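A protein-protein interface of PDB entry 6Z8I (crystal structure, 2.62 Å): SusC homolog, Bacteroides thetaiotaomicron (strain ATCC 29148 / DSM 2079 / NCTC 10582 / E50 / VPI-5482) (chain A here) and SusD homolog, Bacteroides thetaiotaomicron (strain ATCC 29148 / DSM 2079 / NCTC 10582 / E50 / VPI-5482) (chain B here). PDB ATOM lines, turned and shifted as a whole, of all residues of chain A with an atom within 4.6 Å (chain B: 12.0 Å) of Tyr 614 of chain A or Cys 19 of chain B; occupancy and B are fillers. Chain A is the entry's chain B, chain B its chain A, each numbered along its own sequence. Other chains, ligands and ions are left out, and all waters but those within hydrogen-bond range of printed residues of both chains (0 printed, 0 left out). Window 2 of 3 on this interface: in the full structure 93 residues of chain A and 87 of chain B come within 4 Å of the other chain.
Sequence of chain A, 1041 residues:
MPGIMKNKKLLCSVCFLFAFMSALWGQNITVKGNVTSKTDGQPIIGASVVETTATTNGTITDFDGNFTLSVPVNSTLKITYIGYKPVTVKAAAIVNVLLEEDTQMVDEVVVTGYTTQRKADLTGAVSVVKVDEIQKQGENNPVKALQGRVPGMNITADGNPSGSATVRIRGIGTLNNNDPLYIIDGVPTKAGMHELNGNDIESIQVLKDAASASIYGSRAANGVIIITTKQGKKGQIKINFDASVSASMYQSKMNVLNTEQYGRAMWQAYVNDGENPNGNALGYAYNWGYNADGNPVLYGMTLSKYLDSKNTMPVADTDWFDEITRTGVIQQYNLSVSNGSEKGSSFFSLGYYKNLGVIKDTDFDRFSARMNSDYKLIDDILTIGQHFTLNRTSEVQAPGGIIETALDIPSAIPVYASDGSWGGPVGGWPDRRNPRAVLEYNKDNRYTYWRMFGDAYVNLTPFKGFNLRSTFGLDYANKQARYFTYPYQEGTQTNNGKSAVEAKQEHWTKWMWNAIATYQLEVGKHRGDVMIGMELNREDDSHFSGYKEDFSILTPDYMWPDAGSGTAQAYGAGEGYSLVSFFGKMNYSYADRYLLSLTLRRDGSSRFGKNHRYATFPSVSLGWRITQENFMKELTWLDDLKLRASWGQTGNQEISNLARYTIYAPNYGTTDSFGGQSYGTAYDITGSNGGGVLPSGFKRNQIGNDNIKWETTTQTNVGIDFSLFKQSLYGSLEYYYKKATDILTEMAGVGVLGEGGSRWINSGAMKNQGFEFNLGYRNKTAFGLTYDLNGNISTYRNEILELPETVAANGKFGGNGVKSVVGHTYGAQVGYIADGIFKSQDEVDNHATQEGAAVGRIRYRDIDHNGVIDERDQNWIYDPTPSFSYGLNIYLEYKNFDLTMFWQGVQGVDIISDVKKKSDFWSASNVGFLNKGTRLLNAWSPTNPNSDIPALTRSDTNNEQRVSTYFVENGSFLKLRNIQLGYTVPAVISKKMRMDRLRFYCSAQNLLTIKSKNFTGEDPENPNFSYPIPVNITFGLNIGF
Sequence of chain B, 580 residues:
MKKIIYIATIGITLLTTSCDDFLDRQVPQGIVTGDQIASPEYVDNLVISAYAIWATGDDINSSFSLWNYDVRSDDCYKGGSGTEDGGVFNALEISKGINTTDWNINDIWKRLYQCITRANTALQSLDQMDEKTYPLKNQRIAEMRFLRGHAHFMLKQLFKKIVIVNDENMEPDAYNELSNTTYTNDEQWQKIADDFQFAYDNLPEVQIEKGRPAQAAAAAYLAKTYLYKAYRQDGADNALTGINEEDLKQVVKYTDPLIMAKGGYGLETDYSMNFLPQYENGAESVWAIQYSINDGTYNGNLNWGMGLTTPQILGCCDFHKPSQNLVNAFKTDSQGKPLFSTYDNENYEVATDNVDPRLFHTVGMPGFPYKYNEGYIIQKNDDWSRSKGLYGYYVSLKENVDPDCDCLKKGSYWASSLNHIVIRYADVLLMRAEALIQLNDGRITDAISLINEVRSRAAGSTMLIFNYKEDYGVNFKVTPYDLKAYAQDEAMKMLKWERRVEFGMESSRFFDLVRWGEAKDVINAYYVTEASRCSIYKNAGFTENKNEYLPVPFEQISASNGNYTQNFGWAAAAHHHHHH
The backbone carbonyl oxygen (O) of Cys 19 of chain B is in hydrogen-bond range of the side-chain hydroxyl (OH) of Tyr 614 of chain A.
NH2 of Arg 613 of chain A is in salt-bridge range of OD2 of Asp 24 of chain B, at 2.6 Å.
OD1 of Asp 21 of chain B is in hydrogen-bond range of N of Cys 19 of chain B.
N of Gly 604 of chain A sits at hydrogen-bond distance from O of Val 580 of chain A (2.7 Å).
The backbone carbonyl oxygen (O) of Arg 613 of chain A sits at hydrogen-bond distance from the indole nitrogen (NE1) of Trp 710 of chain A.
Phe 22 of chain B touches Leu 536 of chain A.
Leu 23 of chain B touches Val 580 of chain A.
Gly 604 of chain A touches Leu 23 of chain B.
Arg 613 of chain A touches Leu 23 of chain B.
Asp 20 of chain B touches Tyr 614 of chain A.
OH of Tyr 614 of chain A touches CD1 of Leu 23 of chain B, 3.6 Å away.
Hydrophobic or aromatic side chains of chain A within 4 Å of the printed part of chain B: Leu 536, Val 580 and Tyr 614.
Hydrophobic or aromatic side chains of chain B within 4 Å of the printed part of chain A: Phe 22 and Leu 23.
Among the printed residues, Asp or Glu carboxylates within 4 Å of a Lys or Arg side-chain nitrogen of the other chain: Arg 613 of chain A with Asp 24 of chain B (2.6 Å).
Printed residues of chain B within 4 Å of Leu 536 of chain A: Phe 22.
Of chain B, only Leu 23 comes within 4 Å of Val 580 of chain A.
No residue of chain B comes within 4 Å of Arg 602 of chain A.
Of the printed residues of chain B, Gly 604 of chain A touches Leu 23 (3.9 Å).
Printed residues of chain B within 4 Å of Arg 613 of chain A: Leu 23 and Asp 24.
Tyr 614 of chain A touches just these residues of chain B: Cys 19 (3.2 Å), Asp 20 (3.8 Å) and Leu 23 (3.6 Å).
No residue of chain B comes within 4 Å of Ala 615 of chain A.
Cys 19 of chain B touches one residue of chain A.
Printed residues of chain A within 4 Å of Asp 20 of chain B: Tyr 614 (3.8 Å).
Of the printed residues of chain A, Phe 22 of chain B touches Leu 536.
Of the printed residues of chain A, Leu 23 of chain B touches Val 580 (3.5 Å), Gly 604 (3.9 Å), Arg 613 (3.4 Å) and Tyr 614 (3.6 Å).
The nearest printed residue of chain A that does not touch Asp 20 of chain B is Arg 613 of chain A (4.9 Å).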
ATOM      1  N   LEU A 536      -5.443  20.100 -17.478  1.00  0.00           N
ATOM      2  CA  LEU A 536      -5.634  19.877 -18.903  1.00  0.00           C
ATOM      3  C   LEU A 536      -4.276  19.871 -19.593  1.00  0.00           C
ATOM      4  O   LEU A 536      -3.417  20.705 -19.288  1.00  0.00           O
ATOM      5  CB  LEU A 536      -6.521  20.966 -19.515  1.00  0.00           C
ATOM      6  CG  LEU A 536      -7.864  21.253 -18.851  1.00  0.00           C
ATOM      7  CD1 LEU A 536      -8.637  22.332 -19.593  1.00  0.00           C
ATOM      8  CD2 LEU A 536      -8.702  19.976 -18.728  1.00  0.00           C
ATOM      9  N   VAL A 580      -7.038  15.105 -19.827  1.00  0.00           N
ATOM     10  CA  VAL A 580      -7.675  15.740 -18.682  1.00  0.00           C
ATOM     11  C   VAL A 580      -7.397  14.882 -17.459  1.00  0.00           C
ATOM     12  O   VAL A 580      -7.296  13.653 -17.542  1.00  0.00           O
ATOM     13  CB  VAL A 580      -9.189  15.960 -18.892  1.00  0.00           C
ATOM     14  CG1 VAL A 580      -9.853  14.669 -19.182  1.00  0.00           C
ATOM     15  CG2 VAL A 580      -9.839  16.604 -17.677  1.00  0.00           C
ATOM     16  N   PHE A 582      -8.070  14.762 -13.070  1.00  0.00           N
ATOM     17  CA  PHE A 582      -8.643  15.223 -11.810  1.00  0.00           C
ATOM     18  C   PHE A 582      -8.028  14.417 -10.684  1.00  0.00           C
ATOM     19  O   PHE A 582      -7.905  13.194 -10.797  1.00  0.00           O
ATOM     20  CB  PHE A 582     -10.160  15.047 -11.749  1.00  0.00           C
ATOM     21  CG  PHE A 582     -10.895  15.709 -12.855  1.00  0.00           C
ATOM     22  CD1 PHE A 582     -11.114  15.036 -14.056  1.00  0.00           C
ATOM     23  CD2 PHE A 582     -11.394  16.997 -12.702  1.00  0.00           C
ATOM     24  CE1 PHE A 582     -11.808  15.646 -15.090  1.00  0.00           C
ATOM     25  CE2 PHE A 582     -12.080  17.614 -13.735  1.00  0.00           C
ATOM     26  CZ  PHE A 582     -12.293  16.933 -14.931  1.00  0.00           C
ATOM     27  N   ARG A 602      -8.697  10.646 -11.509  1.00  0.00           N
ATOM     28  CA  ARG A 602      -9.345  10.289 -12.783  1.00  0.00           C
ATOM     29  C   ARG A 602      -8.504  10.886 -13.903  1.00  0.00           C
ATOM     30  O   ARG A 602      -8.276  12.096 -13.922  1.00  0.00           O
ATOM     31  CB  ARG A 602     -10.793  10.810 -12.892  1.00  0.00           C
ATOM     32  CG  ARG A 602     -11.965   9.767 -12.783  1.00  0.00           C
ATOM     33  CD  ARG A 602     -13.312  10.201 -13.482  1.00  0.00           C
ATOM     34  NE  ARG A 602     -13.946  11.422 -12.943  1.00  0.00           N
ATOM     35  CZ  ARG A 602     -14.648  12.322 -13.653  1.00  0.00           C
ATOM     36  NH1 ARG A 602     -14.847  12.165 -14.972  1.00  0.00           N
ATOM     37  NH2 ARG A 602     -15.159  13.397 -13.038  1.00  0.00           N
ATOM     38  N   ASP A 603      -8.026  10.045 -14.813  1.00  0.00           N
ATOM     39  CA  ASP A 603      -7.277  10.486 -15.990  1.00  0.00           C
ATOM     40  C   ASP A 603      -8.083  10.182 -17.244  1.00  0.00           C
ATOM     41  O   ASP A 603      -8.587   9.061 -17.406  1.00  0.00           O
ATOM     42  CB  ASP A 603      -5.908   9.802 -16.083  1.00  0.00           C
ATOM     43  CG  ASP A 603      -4.903  10.355 -15.082  1.00  0.00           C
ATOM     44  OD1 ASP A 603      -5.090  11.496 -14.615  1.00  0.00           O
ATOM     45  OD2 ASP A 603      -3.928   9.644 -14.756  1.00  0.00           O
ATOM     46  N   GLY A 604      -8.206  11.175 -18.123  1.00  0.00           N
ATOM     47  CA  GLY A 604      -8.850  10.992 -19.409  1.00  0.00           C
ATOM     48  C   GLY A 604      -7.913  11.320 -20.555  1.00  0.00           C
ATOM     49  O   GLY A 604      -7.112  12.255 -20.476  1.00  0.00           O
ATOM     50  N   HIS A 612     -14.107   4.373 -23.011  1.00  0.00           N
ATOM     51  CA  HIS A 612     -13.045   4.055 -22.064  1.00  0.00           C
ATOM     52  C   HIS A 612     -12.165   5.278 -21.771  1.00  0.00           C
ATOM     53  O   HIS A 612     -11.016   5.137 -21.333  1.00  0.00           O
ATOM     54  CB  HIS A 612     -12.213   2.881 -22.565  1.00  0.00           C
ATOM     55  CG  HIS A 612     -12.964   1.583 -22.582  1.00  0.00           C
ATOM     56  ND1 HIS A 612     -13.549   1.074 -23.723  1.00  0.00           N
ATOM     57  CD2 HIS A 612     -13.244   0.703 -21.592  1.00  0.00           C
ATOM     58  CE1 HIS A 612     -14.140  -0.072 -23.440  1.00  0.00           C
ATOM     59  NE2 HIS A 612     -13.967  -0.320 -22.155  1.00  0.00           N
ATOM     60  N   ARG A 613     -12.709   6.483 -21.963  1.00  0.00           N
ATOM     61  CA  ARG A 613     -11.865   7.668 -22.026  1.00  0.00           C
ATOM     62  C   ARG A 613     -11.164   7.934 -20.690  1.00  0.00           C
ATOM     63  O   ARG A 613      -9.965   8.238 -20.664  1.00  0.00           O
ATOM     64  CB  ARG A 613     -12.707   8.864 -22.479  1.00  0.00           C
ATOM     65  CG  ARG A 613     -11.894  10.062 -22.897  1.00  0.00           C
ATOM     66  CD  ARG A 613     -11.726  10.164 -24.396  1.00  0.00           C
ATOM     67  NE  ARG A 613     -12.859  10.852 -25.005  1.00  0.00           N
ATOM     68  CZ  ARG A 613     -13.111  10.872 -26.310  1.00  0.00           C
ATOM     69  NH1 ARG A 613     -12.312  10.244 -27.163  1.00  0.00           N
ATOM     70  NH2 ARG A 613     -14.173  11.518 -26.765  1.00  0.00           N
ATOM     71  N   TYR A 614     -11.885   7.790 -19.573  1.00  0.00           N
ATOM     72  CA  TYR A 614     -11.342   8.020 -18.240  1.00  0.00           C
ATOM     73  C   TYR A 614     -11.087   6.699 -17.517  1.00  0.00           C
ATOM     74  O   TYR A 614     -11.779   5.711 -17.751  1.00  0.00           O
ATOM     75  CB  TYR A 614     -12.289   8.890 -17.403  1.00  0.00           C
ATOM     76  CG  TYR A 614     -12.554  10.275 -17.977  1.00  0.00           C
ATOM     77  CD1 TYR A 614     -13.523  10.478 -18.962  1.00  0.00           C
ATOM     78  CD2 TYR A 614     -11.833  11.385 -17.535  1.00  0.00           C
ATOM     79  CE1 TYR A 614     -13.778  11.750 -19.477  1.00  0.00           C
ATOM     80  CE2 TYR A 614     -12.080  12.648 -18.044  1.00  0.00           C
ATOM     81  CZ  TYR A 614     -13.051  12.831 -19.015  1.00  0.00           C
ATOM     82  OH  TYR A 614     -13.291  14.096 -19.534  1.00  0.00           O
ATOM     83  N   ALA A 615     -10.085   6.690 -16.630  1.00  0.00           N
ATOM     84  CA  ALA A 615      -9.889   5.616 -15.655  1.00  0.00           C
ATOM     85  C   ALA A 615      -9.565   6.214 -14.291  1.00  0.00           C
ATOM     86  O   ALA A 615      -8.913   7.261 -14.215  1.00  0.00           O
ATOM     87  CB  ALA A 615      -8.767   4.658 -16.061  1.00  0.00           C
ATOM     88  N   THR A 616     -10.016   5.562 -13.212  1.00  0.00           N
ATOM     89  CA  THR A 616      -9.869   6.105 -11.865  1.00  0.00           C
ATOM     90  C   THR A 616      -8.888   5.254 -11.067  1.00  0.00           C
ATOM     91  O   THR A 616      -8.976   4.025 -11.086  1.00  0.00           O
ATOM     92  CB  THR A 616     -11.220   6.197 -11.154  1.00  0.00           C
ATOM     93  OG1 THR A 616     -12.198   6.739 -12.050  1.00  0.00           O
ATOM     94  CG2 THR A 616     -11.104   7.130  -9.984  1.00  0.00           C
ATOM     95  N   TRP A 710      -7.638   1.480 -20.981  1.00  0.00           N
ATOM     96  CA  TRP A 710      -6.416   1.726 -20.224  1.00  0.00           C
ATOM     97  C   TRP A 710      -5.769   0.419 -19.782  1.00  0.00           C
ATOM     98  O   TRP A 710      -6.454  -0.498 -19.335  1.00  0.00           O
ATOM     99  CB  TRP A 710      -6.740   2.559 -18.990  1.00  0.00           C
ATOM    100  CG  TRP A 710      -7.029   4.003 -19.242  1.00  0.00           C
ATOM    101  CD1 TRP A 710      -8.186   4.536 -19.730  1.00  0.00           C
ATOM    102  CD2 TRP A 710      -6.156   5.108 -18.980  1.00  0.00           C
ATOM    103  NE1 TRP A 710      -8.083   5.908 -19.806  1.00  0.00           N
ATOM    104  CE2 TRP A 710      -6.844   6.281 -19.354  1.00  0.00           C
ATOM    105  CE3 TRP A 710      -4.850   5.217 -18.480  1.00  0.00           C
ATOM    106  CZ2 TRP A 710      -6.272   7.547 -19.247  1.00  0.00           C
ATOM    107  CZ3 TRP A 710      -4.287   6.465 -18.365  1.00  0.00           C
ATOM    108  CH2 TRP A 710      -4.994   7.619 -18.754  1.00  0.00           C
ATOM    109  N   CYS B  19     -14.450  20.468 -20.397  1.00  0.00           N
ATOM    110  CA  CYS B  19     -13.420  19.450 -20.217  1.00  0.00           C
ATOM    111  C   CYS B  19     -13.954  18.042 -20.485  1.00  0.00           C
ATOM    112  O   CYS B  19     -13.934  17.186 -19.590  1.00  0.00           O
ATOM    113  CB  CYS B  19     -12.835  19.562 -18.817  1.00  0.00           C
ATOM    114  SG  CYS B  19     -12.660  21.302 -18.293  1.00  0.00           S
ATOM    115  N   ASP B  20     -14.464  17.855 -21.717  1.00  0.00           N
ATOM    116  CA  ASP B  20     -14.808  16.576 -22.350  1.00  0.00           C
ATOM    117  C   ASP B  20     -15.119  16.808 -23.841  1.00  0.00           C
ATOM    118  O   ASP B  20     -14.935  15.910 -24.676  1.00  0.00           O
ATOM    119  CB  ASP B  20     -15.968  15.860 -21.620  1.00  0.00           C
ATOM    120  CG  ASP B  20     -17.085  16.806 -21.154  1.00  0.00           C
ATOM    121  OD1 ASP B  20     -16.794  17.918 -20.649  1.00  0.00           O
ATOM    122  OD2 ASP B  20     -18.266  16.414 -21.262  1.00  0.00           O
ATOM    123  N   ASP B  21     -15.612  18.014 -24.172  1.00  0.00           N
ATOM    124  CA  ASP B  21     -15.459  18.622 -25.503  1.00  0.00           C
ATOM    125  C   ASP B  21     -14.001  18.749 -25.903  1.00  0.00           C
ATOM    126  O   ASP B  21     -13.676  18.807 -27.091  1.00  0.00           O
ATOM    127  CB  ASP B  21     -16.055  20.030 -25.494  1.00  0.00           C
ATOM    128  CG  ASP B  21     -15.493  20.894 -24.340  1.00  0.00           C
ATOM    129  OD1 ASP B  21     -15.228  20.346 -23.241  1.00  0.00           O
ATOM    130  OD2 ASP B  21     -15.299  22.116 -24.533  1.00  0.00           O
ATOM    131  N   PHE B  22     -13.132  18.840 -24.908  1.00  0.00           N
ATOM    132  CA  PHE B  22     -11.704  19.046 -25.044  1.00  0.00           C
ATOM    133  C   PHE B  22     -10.992  17.773 -25.484  1.00  0.00           C
ATOM    134  O   PHE B  22      -9.995  17.844 -26.212  1.00  0.00           O
ATOM    135  CB  PHE B  22     -11.199  19.573 -23.688  1.00  0.00           C
ATOM    136  CG  PHE B  22      -9.713  19.645 -23.549  1.00  0.00           C
ATOM    137  CD1 PHE B  22      -9.032  20.802 -23.887  1.00  0.00           C
ATOM    138  CD2 PHE B  22      -8.998  18.569 -23.036  1.00  0.00           C
ATOM    139  CE1 PHE B  22      -7.658  20.873 -23.750  1.00  0.00           C
ATOM    140  CE2 PHE B  22      -7.623  18.631 -22.901  1.00  0.00           C
ATOM    141  CZ  PHE B  22      -6.950  19.781 -23.257  1.00  0.00           C
ATOM    142  N   LEU B  23     -11.492  16.608 -25.064  1.00  0.00           N
ATOM    143  CA  LEU B  23     -10.882  15.331 -25.398  1.00  0.00           C
ATOM    144  C   LEU B  23     -11.290  14.818 -26.757  1.00  0.00           C
ATOM    145  O   LEU B  23     -10.752  13.794 -27.179  1.00  0.00           O
ATOM    146  CB  LEU B  23     -11.247  14.274 -24.365  1.00  0.00           C
ATOM    147  CG  LEU B  23     -10.543  14.367 -23.025  1.00  0.00           C
ATOM    148  CD1 LEU B  23     -11.018  13.228 -22.148  1.00  0.00           C
ATOM    149  CD2 LEU B  23      -9.037  14.337 -23.218  1.00  0.00           C
ATOM    150  N   ASP B  24     -12.212  15.505 -27.442  1.00  0.00           N
ATOM    151  CA  ASP B  24     -12.739  15.088 -28.741  1.00  0.00           C
ATOM    152  C   ASP B  24     -12.283  15.962 -29.912  1.00  0.00           C
ATOM    153  O   ASP B  24     -12.640  15.664 -31.054  1.00  0.00           O
ATOM    154  CB  ASP B  24     -14.276  15.085 -28.697  1.00  0.00           C
ATOM    155  CG  ASP B  24     -14.874  13.690 -28.752  1.00  0.00           C
ATOM    156  OD1 ASP B  24     -16.081  13.562 -28.442  1.00  0.00           O
ATOM    157  OD2 ASP B  24     -14.149  12.727 -29.096  1.00  0.00           O
ATOM    158  N   ARG B  25     -11.528  17.039 -29.671  1.00  0.00           N
ATOM    159  CA  ARG B  25     -11.309  18.031 -30.724  1.00  0.00           C
ATOM    160  C   ARG B  25     -10.363  17.515 -31.804  1.00  0.00           C
ATOM    161  O   ARG B  25     -10.599  17.728 -32.998  1.00  0.00           O
ATOM    162  CB  ARG B  25     -10.774  19.336 -30.119  1.00  0.00           C
ATOM    163  CG  ARG B  25     -11.830  20.442 -29.930  1.00  0.00           C
ATOM    164  CD  ARG B  25     -11.268  21.677 -29.200  1.00  0.00           C
ATOM    165  NE  ARG B  25     -11.796  21.835 -27.840  1.00  0.00           N
ATOM    166  CZ  ARG B  25     -11.445  22.812 -26.998  1.00  0.00           C
ATOM    167  NH1 ARG B  25     -10.560  23.732 -27.370  1.00  0.00           N
ATOM    168  NH2 ARG B  25     -11.979  22.872 -25.780  1.00  0.00           N
ATOM    169  N   GLN B  26      -9.290  16.839 -31.417  1.00  0.00           N
ATOM    170  CA  GLN B  26      -8.270  16.441 -32.373  1.00  0.00           C
ATOM    171  C   GLN B  26      -8.695  15.221 -33.184  1.00  0.00           C
ATOM    172  O   GLN B  26      -9.033  14.172 -32.631  1.00  0.00           O
ATOM    173  CB  GLN B  26      -6.950  16.173 -31.663  1.00  0.00           C
ATOM    174  CG  GLN B  26      -6.308  17.428 -31.138  1.00  0.00           C
ATOM    175  CD  GLN B  26      -5.376  17.148 -29.981  1.00  0.00           C
ATOM    176  OE1 GLN B  26      -5.296  16.031 -29.518  1.00  0.00           O
ATOM    177  NE2 GLN B  26      -4.674  18.165 -29.513  1.00  0.00           N
